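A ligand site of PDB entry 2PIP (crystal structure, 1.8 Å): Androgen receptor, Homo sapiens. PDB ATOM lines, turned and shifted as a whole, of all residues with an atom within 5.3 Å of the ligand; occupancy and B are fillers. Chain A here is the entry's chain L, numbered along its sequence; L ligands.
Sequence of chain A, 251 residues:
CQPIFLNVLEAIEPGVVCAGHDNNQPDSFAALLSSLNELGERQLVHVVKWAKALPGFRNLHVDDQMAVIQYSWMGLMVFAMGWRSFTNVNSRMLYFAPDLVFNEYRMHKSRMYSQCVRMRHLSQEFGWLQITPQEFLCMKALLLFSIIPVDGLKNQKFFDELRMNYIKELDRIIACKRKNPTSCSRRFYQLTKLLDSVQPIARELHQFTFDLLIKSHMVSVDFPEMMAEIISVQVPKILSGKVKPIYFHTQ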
ATOM      1  N   LEU A  33      14.549  -0.747 -26.073  1.00  0.00           N
ATOM      2  CA  LEU A  33      15.665  -0.245 -25.293  1.00  0.00           C
ATOM      3  C   LEU A  33      15.301   1.005 -24.536  1.00  0.00           C
ATOM      4  O   LEU A  33      15.686   1.147 -23.379  1.00  0.00           O
ATOM      5  CB  LEU A  33      16.881   0.021 -26.189  1.00  0.00           C
ATOM      6  CG  LEU A  33      17.883  -1.142 -26.312  1.00  0.00           C
ATOM      7  CD1 LEU A  33      18.437  -1.452 -24.920  1.00  0.00           C
ATOM      8  CD2 LEU A  33      17.230  -2.379 -26.900  1.00  0.00           C
ATOM      9  N   LEU A  36      13.452   0.003 -21.536  1.00  0.00           N
ATOM     10  CA  LEU A  36      14.377  -0.566 -20.568  1.00  0.00           C
ATOM     11  C   LEU A  36      15.103   0.531 -19.813  1.00  0.00           C
ATOM     12  O   LEU A  36      15.253   0.432 -18.603  1.00  0.00           O
ATOM     13  CB  LEU A  36      15.401  -1.481 -21.254  1.00  0.00           C
ATOM     14  CG  LEU A  36      14.902  -2.849 -21.737  1.00  0.00           C
ATOM     15  CD1 LEU A  36      16.007  -3.536 -22.528  1.00  0.00           C
ATOM     16  CD2 LEU A  36      14.462  -3.691 -20.521  1.00  0.00           C
ATOM     17  N   ASN A  37      15.520   1.582 -20.529  1.00  0.00           N
ATOM     18  CA  ASN A  37      16.213   2.716 -19.919  1.00  0.00           C
ATOM     19  C   ASN A  37      15.320   3.437 -18.922  1.00  0.00           C
ATOM     20  O   ASN A  37      15.759   3.715 -17.804  1.00  0.00           O
ATOM     21  CB  ASN A  37      16.705   3.717 -20.982  1.00  0.00           C
ATOM     22  CG  ASN A  37      17.934   3.201 -21.736  1.00  0.00           C
ATOM     23  OD1 ASN A  37      18.639   2.335 -21.234  1.00  0.00           O
ATOM     24  ND2 ASN A  37      18.213   3.758 -22.918  1.00  0.00           N
ATOM     25  N   LEU A  39      12.604   2.291 -17.364  1.00  0.00           N
ATOM     26  CA  LEU A  39      12.404   1.371 -16.249  1.00  0.00           C
ATOM     27  C   LEU A  39      13.639   1.472 -15.325  1.00  0.00           C
ATOM     28  O   LEU A  39      13.537   1.404 -14.097  1.00  0.00           O
ATOM     29  CB  LEU A  39      12.259  -0.067 -16.768  1.00  0.00           C
ATOM     30  CG  LEU A  39      12.277  -1.173 -15.711  1.00  0.00           C
ATOM     31  CD1 LEU A  39      11.096  -1.032 -14.745  1.00  0.00           C
ATOM     32  CD2 LEU A  39      12.242  -2.496 -16.384  1.00  0.00           C
ATOM     33  N   GLY A  40      14.810   1.599 -15.930  1.00  0.00           N
ATOM     34  CA  GLY A  40      16.024   1.708 -15.149  1.00  0.00           C
ATOM     35  C   GLY A  40      16.010   2.925 -14.255  1.00  0.00           C
ATOM     36  O   GLY A  40      16.348   2.828 -13.089  1.00  0.00           O
ATOM     37  N   GLN A  43      13.371   2.523 -11.443  1.00  0.00           N
ATOM     38  CA  GLN A  43      13.900   1.545 -10.500  1.00  0.00           C
ATOM     39  C   GLN A  43      15.043   2.127  -9.680  1.00  0.00           C
ATOM     40  O   GLN A  43      15.111   1.894  -8.477  1.00  0.00           O
ATOM     41  CB  GLN A  43      14.397   0.314 -11.244  1.00  0.00           C
ATOM     42  CG  GLN A  43      13.304  -0.644 -11.668  1.00  0.00           C
ATOM     43  CD  GLN A  43      12.779  -1.453 -10.503  1.00  0.00           C
ATOM     44  OE1 GLN A  43      11.872  -2.283 -10.668  1.00  0.00           O
ATOM     45  NE2 GLN A  43      13.340  -1.218  -9.321  1.00  0.00           N
ATOM     46  N   TRP A  73      24.072  -0.751  -8.952  1.00  0.00           N
ATOM     47  CA  TRP A  73      22.688  -0.726  -9.437  1.00  0.00           C
ATOM     48  C   TRP A  73      22.391  -1.811 -10.478  1.00  0.00           C
ATOM     49  O   TRP A  73      21.399  -2.532 -10.384  1.00  0.00           O
ATOM     50  CB  TRP A  73      22.334   0.668  -9.986  1.00  0.00           C
ATOM     51  CG  TRP A  73      23.095   1.056 -11.234  1.00  0.00           C
ATOM     52  CD1 TRP A  73      24.330   1.634 -11.286  1.00  0.00           C
ATOM     53  CD2 TRP A  73      22.662   0.885 -12.577  1.00  0.00           C
ATOM     54  NE1 TRP A  73      24.698   1.827 -12.585  1.00  0.00           N
ATOM     55  CE2 TRP A  73      23.695   1.377 -13.407  1.00  0.00           C
ATOM     56  CE3 TRP A  73      21.511   0.360 -13.186  1.00  0.00           C
ATOM     57  CZ2 TRP A  73      23.607   1.370 -14.812  1.00  0.00           C
ATOM     58  CZ3 TRP A  73      21.424   0.344 -14.588  1.00  0.00           C
ATOM     59  CH2 TRP A  73      22.476   0.849 -15.383  1.00  0.00           C
ATOM     60  N   MET A  74      23.247  -1.938 -11.480  1.00  0.00           N
ATOM     61  CA  MET A  74      23.063  -2.932 -12.536  1.00  0.00           C
ATOM     62  C   MET A  74      22.890  -4.330 -11.945  1.00  0.00           C
ATOM     63  O   MET A  74      21.927  -5.044 -12.225  1.00  0.00           O
ATOM     64  CB  MET A  74      24.281  -2.974 -13.438  1.00  0.00           C
ATOM     65  CG  MET A  74      24.159  -3.976 -14.605  1.00  0.00           C
ATOM     66  SD  MET A  74      22.783  -3.572 -15.857  1.00  0.00           S
ATOM     67  CE  MET A  74      23.556  -2.270 -16.671  1.00  0.00           C
ATOM     68  N   MET A  77      19.647  -4.783 -10.002  1.00  0.00           N
ATOM     69  CA  MET A  77      18.470  -4.855 -10.863  1.00  0.00           C
ATOM     70  C   MET A  77      18.342  -6.168 -11.626  1.00  0.00           C
ATOM     71  O   MET A  77      17.227  -6.632 -11.851  1.00  0.00           O
ATOM     72  CB  MET A  77      18.506  -3.669 -11.819  1.00  0.00           C
ATOM     73  CG  MET A  77      18.025  -2.402 -11.149  1.00  0.00           C
ATOM     74  SD  MET A  77      18.073  -0.945 -12.124  1.00  0.00           S
ATOM     75  CE  MET A  77      18.426   0.335 -10.837  1.00  0.00           C
ATOM     76  N   VAL A  78      19.466  -6.748 -12.012  1.00  0.00           N
ATOM     77  CA  VAL A  78      19.484  -8.002 -12.735  1.00  0.00           C
ATOM     78  C   VAL A  78      19.093  -9.136 -11.805  1.00  0.00           C
ATOM     79  O   VAL A  78      18.247  -9.963 -12.156  1.00  0.00           O
ATOM     80  CB  VAL A  78      20.873  -8.252 -13.327  1.00  0.00           C
ATOM     81  CG1 VAL A  78      20.971  -9.731 -13.780  1.00  0.00           C
ATOM     82  CG2 VAL A  78      21.074  -7.329 -14.546  1.00  0.00           C
ATOM     83  N   MET A  81      15.539  -8.879 -11.157  1.00  0.00           N
ATOM     84  CA  MET A  81      14.757  -9.157 -12.345  1.00  0.00           C
ATOM     85  C   MET A  81      14.705 -10.674 -12.528  1.00  0.00           C
ATOM     86  O   MET A  81      13.648 -11.235 -12.877  1.00  0.00           O
ATOM     87  CB  MET A  81      15.395  -8.480 -13.569  1.00  0.00           C
ATOM     88  CG  MET A  81      14.646  -8.694 -14.889  1.00  0.00           C
ATOM     89  SD  MET A  81      14.923 -10.336 -15.747  1.00  0.00           S
ATOM     90  CE  MET A  81      16.390 -10.474 -15.988  1.00  0.00           C
ATOM     91  N   ARG A  84      12.121 -12.268 -10.131  1.00  0.00           N
ATOM     92  CA  ARG A  84      10.738 -12.077 -10.549  1.00  0.00           C
ATOM     93  C   ARG A  84      10.382 -13.067 -11.664  1.00  0.00           C
ATOM     94  O   ARG A  84       9.285 -13.648 -11.681  1.00  0.00           O
ATOM     95  CB  ARG A  84      10.555 -10.633 -11.076  1.00  0.00           C
ATOM     96  CG  ARG A  84      10.740  -9.568 -10.068  1.00  0.00           C
ATOM     97  CD  ARG A  84      10.148  -8.255 -10.518  1.00  0.00           C
ATOM     98  NE  ARG A  84      10.891  -7.615 -11.606  1.00  0.00           N
ATOM     99  CZ  ARG A  84      11.933  -6.808 -11.426  1.00  0.00           C
ATOM    100  NH1 ARG A  84      12.388  -6.516 -10.229  1.00  0.00           N
ATOM    101  NH2 ARG A  84      12.571  -6.300 -12.458  1.00  0.00           N
ATOM    102  N   PHE A  96      11.009  -8.186 -16.770  1.00  0.00           N
ATOM    103  CA  PHE A  96      11.527  -6.858 -16.444  1.00  0.00           C
ATOM    104  C   PHE A  96      10.521  -6.050 -15.626  1.00  0.00           C
ATOM    105  O   PHE A  96      10.879  -5.422 -14.636  1.00  0.00           O
ATOM    106  CB  PHE A  96      11.878  -6.103 -17.724  1.00  0.00           C
ATOM    107  CG  PHE A  96      13.086  -6.635 -18.410  1.00  0.00           C
ATOM    108  CD1 PHE A  96      14.358  -6.540 -17.833  1.00  0.00           C
ATOM    109  CD2 PHE A  96      12.967  -7.275 -19.643  1.00  0.00           C
ATOM    110  CE1 PHE A  96      15.500  -7.065 -18.488  1.00  0.00           C
ATOM    111  CE2 PHE A  96      14.101  -7.800 -20.291  1.00  0.00           C
ATOM    112  CZ  PHE A  96      15.356  -7.695 -19.704  1.00  0.00           C
ATOM    113  N   MET A 112      20.446  -7.793 -27.838  1.00  0.00           N
ATOM    114  CA  MET A 112      21.243  -8.209 -26.693  1.00  0.00           C
ATOM    115  C   MET A 112      20.759  -9.583 -26.257  1.00  0.00           C
ATOM    116  O   MET A 112      20.567  -9.849 -25.072  1.00  0.00           O
ATOM    117  CB  MET A 112      21.136  -7.213 -25.542  1.00  0.00           C
ATOM    118  CG  MET A 112      19.750  -6.998 -25.079  1.00  0.00           C
ATOM    119  SD  MET A 112      19.655  -5.758 -23.706  1.00  0.00           S
ATOM    120  CE  MET A 112      19.276  -6.854 -22.345  1.00  0.00           C
ATOM    121  N   MET A 119      21.130 -13.817 -18.408  1.00  0.00           N
ATOM    122  CA  MET A 119      20.261 -13.373 -17.322  1.00  0.00           C
ATOM    123  C   MET A 119      19.162 -14.415 -17.056  1.00  0.00           C
ATOM    124  O   MET A 119      18.798 -14.682 -15.913  1.00  0.00           O
ATOM    125  CB  MET A 119      19.630 -12.023 -17.653  1.00  0.00           C
ATOM    126  CG  MET A 119      20.576 -10.847 -17.709  1.00  0.00           C
ATOM    127  SD  MET A 119      19.554  -9.315 -17.993  1.00  0.00           S
ATOM    128  CE  MET A 119      19.477  -9.501 -19.900  1.00  0.00           C
ATOM    129  N   LEU A 205      26.534  -6.100 -19.453  1.00  0.00           N
ATOM    130  CA  LEU A 205      25.450  -5.150 -19.588  1.00  0.00           C
ATOM    131  C   LEU A 205      26.030  -3.745 -19.483  1.00  0.00           C
ATOM    132  O   LEU A 205      25.503  -2.821 -20.089  1.00  0.00           O
ATOM    133  CB  LEU A 205      24.395  -5.374 -18.501  1.00  0.00           C
ATOM    134  CG  LEU A 205      23.490  -6.617 -18.710  1.00  0.00           C
ATOM    135  CD1 LEU A 205      22.633  -6.874 -17.533  1.00  0.00           C
ATOM    136  CD2 LEU A 205      22.670  -6.513 -19.979  1.00  0.00           C
ATOM    137  N   PHE A 208      27.522  -3.013 -22.834  1.00  0.00           N
ATOM    138  CA  PHE A 208      26.452  -2.842 -23.803  1.00  0.00           C
ATOM    139  C   PHE A 208      25.747  -1.504 -23.674  1.00  0.00           C
ATOM    140  O   PHE A 208      25.564  -0.781 -24.664  1.00  0.00           O
ATOM    141  CB  PHE A 208      25.441  -3.989 -23.672  1.00  0.00           C
ATOM    142  CG  PHE A 208      24.380  -3.966 -24.726  1.00  0.00           C
ATOM    143  CD1 PHE A 208      23.219  -3.210 -24.558  1.00  0.00           C
ATOM    144  CD2 PHE A 208      24.547  -4.715 -25.901  1.00  0.00           C
ATOM    145  CE1 PHE A 208      22.237  -3.188 -25.554  1.00  0.00           C
ATOM    146  CE2 PHE A 208      23.574  -4.703 -26.901  1.00  0.00           C
ATOM    147  CZ  PHE A 208      22.418  -3.935 -26.729  1.00  0.00           C
ATOM    148  N   THR A 209      25.394  -1.133 -22.442  1.00  0.00           N
ATOM    149  CA  THR A 209      24.693   0.137 -22.215  1.00  0.00           C
ATOM    150  C   THR A 209      25.598   1.332 -22.557  1.00  0.00           C
ATOM    151  O   THR A 209      25.146   2.313 -23.159  1.00  0.00           O
ATOM    152  CB  THR A 209      24.208   0.263 -20.752  1.00  0.00           C
ATOM    153  OG1 THR A 209      23.436   1.461 -20.584  1.00  0.00           O
ATOM    154  CG2 THR A 209      25.426   0.299 -19.782  1.00  0.00           C
ATOM    155  N   LEU A 212      25.702   1.750 -26.165  1.00  0.00           N
ATOM    156  CA  LEU A 212      24.408   2.226 -26.608  1.00  0.00           C
ATOM    157  C   LEU A 212      24.283   3.722 -26.382  1.00  0.00           C
ATOM    158  O   LEU A 212      23.723   4.437 -27.222  1.00  0.00           O
ATOM    159  CB  LEU A 212      23.270   1.512 -25.897  1.00  0.00           C
ATOM    160  CG  LEU A 212      21.833   1.868 -26.297  1.00  0.00           C
ATOM    161  CD1 LEU A 212      21.638   1.682 -27.780  1.00  0.00           C
ATOM    162  CD2 LEU A 212      20.878   0.983 -25.490  1.00  0.00           C
ATOM    163  N   PHE A 223      17.735   8.018 -23.361  1.00  0.00           N
ATOM    164  CA  PHE A 223      18.339   7.724 -22.064  1.00  0.00           C
ATOM    165  C   PHE A 223      17.899   8.740 -21.031  1.00  0.00           C
ATOM    166  O   PHE A 223      18.130   9.936 -21.212  1.00  0.00           O
ATOM    167  CB  PHE A 223      19.862   7.756 -22.149  1.00  0.00           C
ATOM    168  CG  PHE A 223      20.477   6.472 -22.592  1.00  0.00           C
ATOM    169  CD1 PHE A 223      20.468   6.094 -23.945  1.00  0.00           C
ATOM    170  CD2 PHE A 223      21.084   5.619 -21.675  1.00  0.00           C
ATOM    171  CE1 PHE A 223      21.055   4.875 -24.363  1.00  0.00           C
ATOM    172  CE2 PHE A 223      21.678   4.397 -22.071  1.00  0.00           C
ATOM    173  CZ  PHE A 223      21.666   4.032 -23.412  1.00  0.00           C
ATOM    174  N   ILE A 231      25.958   6.303 -16.430  1.00  0.00           N
ATOM    175  CA  ILE A 231      26.599   5.470 -17.430  1.00  0.00           C
ATOM    176  C   ILE A 231      27.798   6.164 -18.103  1.00  0.00           C
ATOM    177  O   ILE A 231      28.704   5.497 -18.577  1.00  0.00           O
ATOM    178  CB  ILE A 231      25.588   5.060 -18.520  1.00  0.00           C
ATOM    179  CG1 ILE A 231      24.415   4.310 -17.875  1.00  0.00           C
ATOM    180  CG2 ILE A 231      26.281   4.183 -19.564  1.00  0.00           C
ATOM    181  CD1 ILE A 231      23.218   4.127 -18.782  1.00  0.00           C
HETATM  182  C1  LIG L   1      16.132  -2.322 -15.903  1.00  0.00           C
HETATM  183  C2  LIG L   1      15.691  -2.844 -14.559  1.00  0.00           C
HETATM  184  C3  LIG L   1      15.532  -4.409 -14.692  1.00  0.00           C
HETATM  185  O1  LIG L   1      14.572  -4.951 -14.394  1.00  0.00           O
HETATM  186  C4  LIG L   1      16.769  -5.108 -15.200  1.00  0.00           C
HETATM  187  C5  LIG L   1      17.241  -4.521 -16.558  1.00  0.00           C
HETATM  188  C6  LIG L   1      18.545  -5.223 -17.125  1.00  0.00           C
HETATM  189  C7  LIG L   1      18.931  -4.602 -18.492  1.00  0.00           C
HETATM  190  C8  LIG L   1      19.169  -3.057 -18.450  1.00  0.00           C
HETATM  191  C9  LIG L   1      17.875  -2.406 -17.883  1.00  0.00           C
HETATM  192  C10 LIG L   1      17.449  -2.947 -16.430  1.00  0.00           C
HETATM  193  C11 LIG L   1      18.142  -0.832 -17.868  1.00  0.00           C
HETATM  194  C12 LIG L   1      18.528  -0.213 -19.205  1.00  0.00           C
HETATM  195  C13 LIG L   1      19.737  -0.933 -19.848  1.00  0.00           C
HETATM  196  C14 LIG L   1      19.478  -2.482 -19.854  1.00  0.00           C
HETATM  197  C15 LIG L   1      20.735  -3.001 -20.562  1.00  0.00           C
HETATM  198  C16 LIG L   1      20.884  -2.002 -21.738  1.00  0.00           C
HETATM  199  C17 LIG L   1      19.968  -0.793 -21.357  1.00  0.00           C
HETATM  200  O2  LIG L   1      20.626   0.414 -21.677  1.00  0.00           O
HETATM  201  C18 LIG L   1      21.053  -0.541 -19.031  1.00  0.00           C
HETATM  202  C19 LIG L   1      18.604  -2.638 -15.384  1.00  0.00           C
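O2 of the ligand is in hydrogen-bond range of OD1 of Asn 37, 2.8 Å away.
O1 of the ligand sits at hydrogen-bond distance from NH2 of Arg 84, 3.1 Å away.
An oxygen (O2) of the ligand is in hydrogen-bond range of the side-chain hydroxyl (OG1) of Thr 209.
The guanidinium group of Arg 84 lies within hydrogen-bond range of the backbone carbonyl oxygen of Phe 96 (2.9 Å).
Merely in contact with the ligand: Leu 36 (3.2 Å), Phe 96 (3.6 Å), Met 77 (3.7 Å), Met 81 (3.7 Å), Met 74 (3.9 Å), Phe 208 (3.9 Å), Leu 212 (3.9 Å), Leu 39 (3.9 Å) and Leu 33 (3.9 Å).
Hydrophobic or aromatic side chains that line the ligand: Leu 33, Leu 36, Leu 39, Met 74, Met 77, Met 81, Phe 96, Phe 208 and Leu 212.
12 residues have an atom within 4 Å of the ligand: Leu 33, Leu 36, Asn 37, Leu 39, Met 74, Met 77, Met 81, Arg 84, Phe 96, Phe 208, Thr 209 and Leu 212.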
